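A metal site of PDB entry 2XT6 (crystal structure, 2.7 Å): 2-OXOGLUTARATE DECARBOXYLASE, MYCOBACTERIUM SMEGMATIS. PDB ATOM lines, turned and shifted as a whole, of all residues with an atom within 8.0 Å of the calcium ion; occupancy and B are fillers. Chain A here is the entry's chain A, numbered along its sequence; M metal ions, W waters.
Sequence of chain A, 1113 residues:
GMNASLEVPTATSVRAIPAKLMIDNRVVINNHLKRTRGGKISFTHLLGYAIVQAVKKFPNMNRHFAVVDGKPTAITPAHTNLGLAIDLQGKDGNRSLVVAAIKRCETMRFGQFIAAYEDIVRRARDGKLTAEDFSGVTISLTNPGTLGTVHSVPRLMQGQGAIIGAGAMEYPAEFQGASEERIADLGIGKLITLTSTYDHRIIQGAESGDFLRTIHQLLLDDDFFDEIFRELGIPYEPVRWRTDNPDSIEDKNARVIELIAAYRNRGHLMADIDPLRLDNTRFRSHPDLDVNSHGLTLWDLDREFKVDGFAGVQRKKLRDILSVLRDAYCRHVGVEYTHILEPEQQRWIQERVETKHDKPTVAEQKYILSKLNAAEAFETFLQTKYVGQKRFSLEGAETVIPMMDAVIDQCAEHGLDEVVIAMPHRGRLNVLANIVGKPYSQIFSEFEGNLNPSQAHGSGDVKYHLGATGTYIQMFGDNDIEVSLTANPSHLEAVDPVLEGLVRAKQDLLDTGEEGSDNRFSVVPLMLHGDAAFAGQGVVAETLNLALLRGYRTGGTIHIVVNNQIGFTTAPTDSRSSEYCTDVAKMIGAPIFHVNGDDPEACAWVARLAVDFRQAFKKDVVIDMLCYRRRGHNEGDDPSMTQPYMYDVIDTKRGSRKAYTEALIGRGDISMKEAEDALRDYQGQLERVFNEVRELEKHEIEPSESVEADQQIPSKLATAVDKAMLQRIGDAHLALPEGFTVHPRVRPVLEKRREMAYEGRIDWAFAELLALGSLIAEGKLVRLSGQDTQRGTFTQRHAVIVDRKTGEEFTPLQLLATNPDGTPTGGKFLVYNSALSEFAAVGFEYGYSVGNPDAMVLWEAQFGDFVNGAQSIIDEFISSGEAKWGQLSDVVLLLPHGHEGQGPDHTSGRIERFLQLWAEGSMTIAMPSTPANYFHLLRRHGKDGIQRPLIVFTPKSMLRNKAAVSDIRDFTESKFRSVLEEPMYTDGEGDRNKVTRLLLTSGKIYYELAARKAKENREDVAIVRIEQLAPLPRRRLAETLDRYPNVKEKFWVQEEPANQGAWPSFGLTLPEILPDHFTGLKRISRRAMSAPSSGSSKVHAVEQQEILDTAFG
OD1 of Asp 890 lies close to N of Arg 948.
Four residues have an atom within 4 Å of the calcium ion: Asp 890, His 941, Asp 944 and Ile 946.
The calcium ion is bound by water W1, OD1 of Asp 890, O of Ile 946, OD2 of Asp 944 and O of His 941. The calcium ion has five donor atoms within binding distance. Slightly farther from the calcium ion lies OD1 of Asp 944 (3.1 Å).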
ATOM      1  N   LYS A 780      22.381 -19.334 -21.854  1.00  0.00           N
ATOM      2  CA  LYS A 780      21.195 -18.752 -22.486  1.00  0.00           C
ATOM      3  C   LYS A 780      21.459 -17.418 -23.184  1.00  0.00           C
ATOM      4  O   LYS A 780      22.204 -16.586 -22.658  1.00  0.00           O
ATOM      5  CB  LYS A 780      20.078 -18.543 -21.448  1.00  0.00           C
ATOM      6  CG  LYS A 780      18.672 -18.608 -22.030  1.00  0.00           C
ATOM      7  CD  LYS A 780      17.617 -18.778 -20.961  1.00  0.00           C
ATOM      8  CE  LYS A 780      16.228 -18.774 -21.562  1.00  0.00           C
ATOM      9  NZ  LYS A 780      15.863 -20.084 -22.165  1.00  0.00           N
ATOM     10  N   PRO A 853      12.745 -19.638 -29.535  1.00  0.00           N
ATOM     11  CA  PRO A 853      12.062 -20.020 -28.292  1.00  0.00           C
ATOM     12  C   PRO A 853      12.995 -20.217 -27.098  1.00  0.00           C
ATOM     13  O   PRO A 853      12.537 -20.115 -25.950  1.00  0.00           O
ATOM     14  CB  PRO A 853      11.402 -21.333 -28.674  1.00  0.00           C
ATOM     15  CG  PRO A 853      11.273 -21.275 -30.186  1.00  0.00           C
ATOM     16  CD  PRO A 853      12.555 -20.668 -30.579  1.00  0.00           C
ATOM     17  N   ALA A 855      15.550 -18.225 -26.355  1.00  0.00           N
ATOM     18  CA  ALA A 855      16.082 -16.944 -25.956  1.00  0.00           C
ATOM     19  C   ALA A 855      15.208 -16.338 -24.891  1.00  0.00           C
ATOM     20  O   ALA A 855      13.970 -16.507 -24.918  1.00  0.00           O
ATOM     21  CB  ALA A 855      16.179 -16.017 -27.148  1.00  0.00           C
ATOM     22  N   MET A 856      15.843 -15.673 -23.921  1.00  0.00           N
ATOM     23  CA  MET A 856      15.164 -14.922 -22.871  1.00  0.00           C
ATOM     24  C   MET A 856      15.005 -13.526 -23.459  1.00  0.00           C
ATOM     25  O   MET A 856      16.011 -12.848 -23.667  1.00  0.00           O
ATOM     26  CB  MET A 856      15.971 -14.960 -21.553  1.00  0.00           C
ATOM     27  CG  MET A 856      15.437 -14.070 -20.478  1.00  0.00           C
ATOM     28  SD  MET A 856      14.206 -14.890 -19.443  1.00  0.00           S
ATOM     29  CE  MET A 856      13.691 -13.503 -18.410  1.00  0.00           C
ATOM     30  N   SER A 889       4.864 -17.654 -27.566  1.00  0.00           N
ATOM     31  CA  SER A 889       5.859 -16.588 -27.326  1.00  0.00           C
ATOM     32  C   SER A 889       6.206 -16.552 -25.848  1.00  0.00           C
ATOM     33  O   SER A 889       5.330 -16.746 -25.022  1.00  0.00           O
ATOM     34  CB  SER A 889       5.333 -15.249 -27.786  1.00  0.00           C
ATOM     35  OG  SER A 889       6.149 -14.158 -27.399  1.00  0.00           O
ATOM     36  N   ASP A 890       7.481 -16.330 -25.513  1.00  0.00           N
ATOM     37  CA  ASP A 890       7.948 -16.273 -24.122  1.00  0.00           C
ATOM     38  C   ASP A 890       8.409 -14.851 -23.792  1.00  0.00           C
ATOM     39  O   ASP A 890       9.268 -14.658 -22.920  1.00  0.00           O
ATOM     40  CB  ASP A 890       9.076 -17.302 -23.913  1.00  0.00           C
ATOM     41  CG  ASP A 890       9.214 -17.804 -22.487  1.00  0.00           C
ATOM     42  OD1 ASP A 890       8.197 -18.196 -21.888  1.00  0.00           O
ATOM     43  OD2 ASP A 890      10.381 -17.865 -21.988  1.00  0.00           O
ATOM     44  N   VAL A 891       7.871 -13.848 -24.509  1.00  0.00           N
ATOM     45  CA  VAL A 891       8.254 -12.443 -24.354  1.00  0.00           C
ATOM     46  C   VAL A 891       7.914 -11.949 -22.935  1.00  0.00           C
ATOM     47  O   VAL A 891       6.903 -12.370 -22.353  1.00  0.00           O
ATOM     48  CB  VAL A 891       7.654 -11.523 -25.465  1.00  0.00           C
ATOM     49  CG1 VAL A 891       6.156 -11.233 -25.254  1.00  0.00           C
ATOM     50  CG2 VAL A 891       8.454 -10.227 -25.620  1.00  0.00           C
ATOM     51  N   VAL A 892       8.802 -11.079 -22.388  1.00  0.00           N
ATOM     52  CA  VAL A 892       8.637 -10.426 -21.096  1.00  0.00           C
ATOM     53  C   VAL A 892       8.426  -8.951 -21.336  1.00  0.00           C
ATOM     54  O   VAL A 892       9.287  -8.303 -21.957  1.00  0.00           O
ATOM     55  CB  VAL A 892       9.791 -10.645 -20.096  1.00  0.00           C
ATOM     56  CG1 VAL A 892       9.380 -10.197 -18.697  1.00  0.00           C
ATOM     57  CG2 VAL A 892      10.243 -12.079 -20.083  1.00  0.00           C
ATOM     58  N   THR A 924       1.413 -14.814 -17.935  1.00  0.00           N
ATOM     59  CA  THR A 924       1.682 -14.735 -16.501  1.00  0.00           C
ATOM     60  C   THR A 924       1.735 -13.253 -16.191  1.00  0.00           C
ATOM     61  O   THR A 924       2.353 -12.502 -16.949  1.00  0.00           O
ATOM     62  CB  THR A 924       2.967 -15.479 -16.092  1.00  0.00           C
ATOM     63  OG1 THR A 924       3.014 -16.761 -16.721  1.00  0.00           O
ATOM     64  CG2 THR A 924       3.088 -15.623 -14.600  1.00  0.00           C
ATOM     65  N   LEU A 937      11.342 -15.159 -10.385  1.00  0.00           N
ATOM     66  CA  LEU A 937      10.315 -15.027 -11.397  1.00  0.00           C
ATOM     67  C   LEU A 937      10.911 -15.067 -12.811  1.00  0.00           C
ATOM     68  O   LEU A 937      10.362 -15.756 -13.673  1.00  0.00           O
ATOM     69  CB  LEU A 937       9.531 -13.706 -11.189  1.00  0.00           C
ATOM     70  CG  LEU A 937       8.457 -13.358 -12.204  1.00  0.00           C
ATOM     71  CD1 LEU A 937       7.217 -14.228 -12.009  1.00  0.00           C
ATOM     72  CD2 LEU A 937       8.095 -11.939 -12.090  1.00  0.00           C
ATOM     73  N   LEU A 938      12.022 -14.322 -13.050  1.00  0.00           N
ATOM     74  CA  LEU A 938      12.735 -14.245 -14.341  1.00  0.00           C
ATOM     75  C   LEU A 938      13.409 -15.569 -14.666  1.00  0.00           C
ATOM     76  O   LEU A 938      13.362 -16.025 -15.815  1.00  0.00           O
ATOM     77  CB  LEU A 938      13.792 -13.114 -14.352  1.00  0.00           C
ATOM     78  CG  LEU A 938      13.299 -11.647 -14.311  1.00  0.00           C
ATOM     79  CD1 LEU A 938      14.470 -10.706 -14.222  1.00  0.00           C
ATOM     80  CD2 LEU A 938      12.479 -11.296 -15.518  1.00  0.00           C
ATOM     81  N   ARG A 939      14.024 -16.189 -13.645  1.00  0.00           N
ATOM     82  CA  ARG A 939      14.705 -17.471 -13.783  1.00  0.00           C
ATOM     83  C   ARG A 939      13.676 -18.541 -14.076  1.00  0.00           C
ATOM     84  O   ARG A 939      13.925 -19.340 -14.969  1.00  0.00           O
ATOM     85  CB  ARG A 939      15.512 -17.821 -12.501  1.00  0.00           C
ATOM     86  CG  ARG A 939      16.590 -16.822 -12.103  1.00  0.00           C
ATOM     87  CD  ARG A 939      17.999 -17.258 -12.457  1.00  0.00           C
ATOM     88  NE  ARG A 939      18.319 -18.582 -11.945  1.00  0.00           N
ATOM     89  CZ  ARG A 939      19.077 -19.446 -12.598  1.00  0.00           C
ATOM     90  NH1 ARG A 939      19.612 -19.125 -13.766  1.00  0.00           N
ATOM     91  NH2 ARG A 939      19.305 -20.645 -12.090  1.00  0.00           N
ATOM     92  N   ARG A 940      12.530 -18.549 -13.366  1.00  0.00           N
ATOM     93  CA  ARG A 940      11.476 -19.525 -13.619  1.00  0.00           C
ATOM     94  C   ARG A 940      11.011 -19.405 -15.057  1.00  0.00           C
ATOM     95  O   ARG A 940      10.945 -20.405 -15.780  1.00  0.00           O
ATOM     96  CB  ARG A 940      10.303 -19.343 -12.660  1.00  0.00           C
ATOM     97  CG  ARG A 940       9.199 -20.397 -12.812  1.00  0.00           C
ATOM     98  CD  ARG A 940       7.966 -20.106 -11.969  1.00  0.00           C
ATOM     99  NE  ARG A 940       7.336 -18.854 -12.390  1.00  0.00           N
ATOM    100  CZ  ARG A 940       6.162 -18.406 -11.935  1.00  0.00           C
ATOM    101  NH1 ARG A 940       5.482 -19.112 -11.045  1.00  0.00           N
ATOM    102  NH2 ARG A 940       5.678 -17.264 -12.371  1.00  0.00           N
ATOM    103  N   HIS A 941      10.752 -18.156 -15.499  1.00  0.00           N
ATOM    104  CA  HIS A 941      10.317 -17.833 -16.831  1.00  0.00           C
ATOM    105  C   HIS A 941      11.269 -18.392 -17.923  1.00  0.00           C
ATOM    106  O   HIS A 941      10.818 -19.118 -18.826  1.00  0.00           O
ATOM    107  CB  HIS A 941      10.152 -16.324 -16.974  1.00  0.00           C
ATOM    108  CG  HIS A 941       9.554 -15.933 -18.284  1.00  0.00           C
ATOM    109  ND1 HIS A 941       8.237 -16.218 -18.584  1.00  0.00           N
ATOM    110  CD2 HIS A 941      10.143 -15.398 -19.371  1.00  0.00           C
ATOM    111  CE1 HIS A 941       8.056 -15.796 -19.819  1.00  0.00           C
ATOM    112  NE2 HIS A 941       9.167 -15.284 -20.333  1.00  0.00           N
ATOM    113  N   GLY A 942      12.562 -18.090 -17.801  1.00  0.00           N
ATOM    114  CA  GLY A 942      13.571 -18.538 -18.749  1.00  0.00           C
ATOM    115  C   GLY A 942      13.829 -20.022 -18.755  1.00  0.00           C
ATOM    116  O   GLY A 942      14.200 -20.555 -19.802  1.00  0.00           O
ATOM    117  N   LYS A 943      13.591 -20.719 -17.623  1.00  0.00           N
ATOM    118  CA  LYS A 943      13.923 -22.145 -17.458  1.00  0.00           C
ATOM    119  C   LYS A 943      12.745 -23.164 -17.356  1.00  0.00           C
ATOM    120  O   LYS A 943      13.004 -24.329 -17.117  1.00  0.00           O
ATOM    121  CB  LYS A 943      14.773 -22.298 -16.182  1.00  0.00           C
ATOM    122  CG  LYS A 943      16.104 -21.537 -16.192  1.00  0.00           C
ATOM    123  CD  LYS A 943      16.730 -21.436 -14.793  1.00  0.00           C
ATOM    124  CE  LYS A 943      17.227 -22.731 -14.185  1.00  0.00           C
ATOM    125  NZ  LYS A 943      18.366 -23.319 -14.948  1.00  0.00           N
ATOM    126  N   ASP A 944      11.485 -22.751 -17.503  1.00  0.00           N
ATOM    127  CA  ASP A 944      10.341 -23.654 -17.296  1.00  0.00           C
ATOM    128  C   ASP A 944       9.980 -24.561 -18.486  1.00  0.00           C
ATOM    129  O   ASP A 944       9.136 -25.449 -18.323  1.00  0.00           O
ATOM    130  CB  ASP A 944       9.089 -22.857 -16.885  1.00  0.00           C
ATOM    131  CG  ASP A 944       8.716 -21.672 -17.773  1.00  0.00           C
ATOM    132  OD1 ASP A 944       7.946 -20.808 -17.313  1.00  0.00           O
ATOM    133  OD2 ASP A 944       9.183 -21.630 -18.944  1.00  0.00           O
ATOM    134  N   GLY A 945      10.552 -24.299 -19.668  1.00  0.00           N
ATOM    135  CA  GLY A 945      10.279 -25.061 -20.887  1.00  0.00           C
ATOM    136  C   GLY A 945       8.913 -24.768 -21.485  1.00  0.00           C
ATOM    137  O   GLY A 945       8.461 -25.485 -22.392  1.00  0.00           O
ATOM    138  N   ILE A 946       8.247 -23.709 -20.969  1.00  0.00           N
ATOM    139  CA  ILE A 946       6.920 -23.259 -21.392  1.00  0.00           C
ATOM    140  C   ILE A 946       7.152 -21.974 -22.122  1.00  0.00           C
ATOM    141  O   ILE A 946       7.972 -21.175 -21.676  1.00  0.00           O
ATOM    142  CB  ILE A 946       5.986 -23.097 -20.160  1.00  0.00           C
ATOM    143  CG1 ILE A 946       5.624 -24.454 -19.552  1.00  0.00           C
ATOM    144  CG2 ILE A 946       4.728 -22.296 -20.470  1.00  0.00           C
ATOM    145  CD1 ILE A 946       5.296 -24.370 -17.997  1.00  0.00           C
ATOM    146  N   GLN A 947       6.442 -21.772 -23.231  1.00  0.00           N
ATOM    147  CA  GLN A 947       6.517 -20.543 -24.018  1.00  0.00           C
ATOM    148  C   GLN A 947       5.205 -19.809 -23.814  1.00  0.00           C
ATOM    149  O   GLN A 947       4.215 -20.108 -24.470  1.00  0.00           O
ATOM    150  CB  GLN A 947       6.803 -20.866 -25.492  1.00  0.00           C
ATOM    151  CG  GLN A 947       8.085 -21.655 -25.741  1.00  0.00           C
ATOM    152  CD  GLN A 947       9.294 -20.799 -25.599  1.00  0.00           C
ATOM    153  OE1 GLN A 947       9.436 -19.763 -26.262  1.00  0.00           O
ATOM    154  NE2 GLN A 947      10.183 -21.189 -24.706  1.00  0.00           N
ATOM    155  N   ARG A 948       5.177 -18.927 -22.831  1.00  0.00           N
ATOM    156  CA  ARG A 948       4.005 -18.160 -22.398  1.00  0.00           C
ATOM    157  C   ARG A 948       4.449 -16.758 -21.992  1.00  0.00           C
ATOM    158  O   ARG A 948       5.398 -16.648 -21.213  1.00  0.00           O
ATOM    159  CB  ARG A 948       3.362 -18.900 -21.225  1.00  0.00           C
ATOM    160  CG  ARG A 948       2.085 -18.317 -20.678  1.00  0.00           C
ATOM    161  CD  ARG A 948       1.341 -19.403 -19.918  1.00  0.00           C
ATOM    162  NE  ARG A 948       0.832 -20.428 -20.820  1.00  0.00           N
ATOM    163  CZ  ARG A 948       0.689 -21.709 -20.505  1.00  0.00           C
ATOM    164  NH1 ARG A 948       1.026 -22.133 -19.292  1.00  0.00           N
ATOM    165  NH2 ARG A 948       0.207 -22.569 -21.387  1.00  0.00           N
ATOM    166  N   PRO A 949       3.843 -15.660 -22.489  1.00  0.00           N
ATOM    167  CA  PRO A 949       4.363 -14.328 -22.146  1.00  0.00           C
ATOM    168  C   PRO A 949       4.222 -14.018 -20.667  1.00  0.00           C
ATOM    169  O   PRO A 949       3.355 -14.534 -19.971  1.00  0.00           O
ATOM    170  CB  PRO A 949       3.514 -13.377 -22.994  1.00  0.00           C
ATOM    171  CG  PRO A 949       2.974 -14.200 -24.078  1.00  0.00           C
ATOM    172  CD  PRO A 949       2.712 -15.536 -23.434  1.00  0.00           C
ATOM    173  N   LEU A 950       5.132 -13.168 -20.192  1.00  0.00           N
ATOM    174  CA  LEU A 950       5.147 -12.698 -18.813  1.00  0.00           C
ATOM    175  C   LEU A 950       5.068 -11.188 -18.819  1.00  0.00           C
ATOM    176  O   LEU A 950       5.825 -10.511 -19.538  1.00  0.00           O
ATOM    177  CB  LEU A 950       6.392 -13.219 -18.054  1.00  0.00           C
ATOM    178  CG  LEU A 950       6.709 -12.585 -16.658  1.00  0.00           C
ATOM    179  CD1 LEU A 950       5.699 -12.944 -15.598  1.00  0.00           C
ATOM    180  CD2 LEU A 950       8.118 -12.978 -16.165  1.00  0.00           C
HETATM  181 CA    CA M   1       8.404 -19.411 -20.005  1.00  0.00          CA
HETATM  182  O   HOH W   1      10.073 -20.260 -21.035  1.00  0.00           O
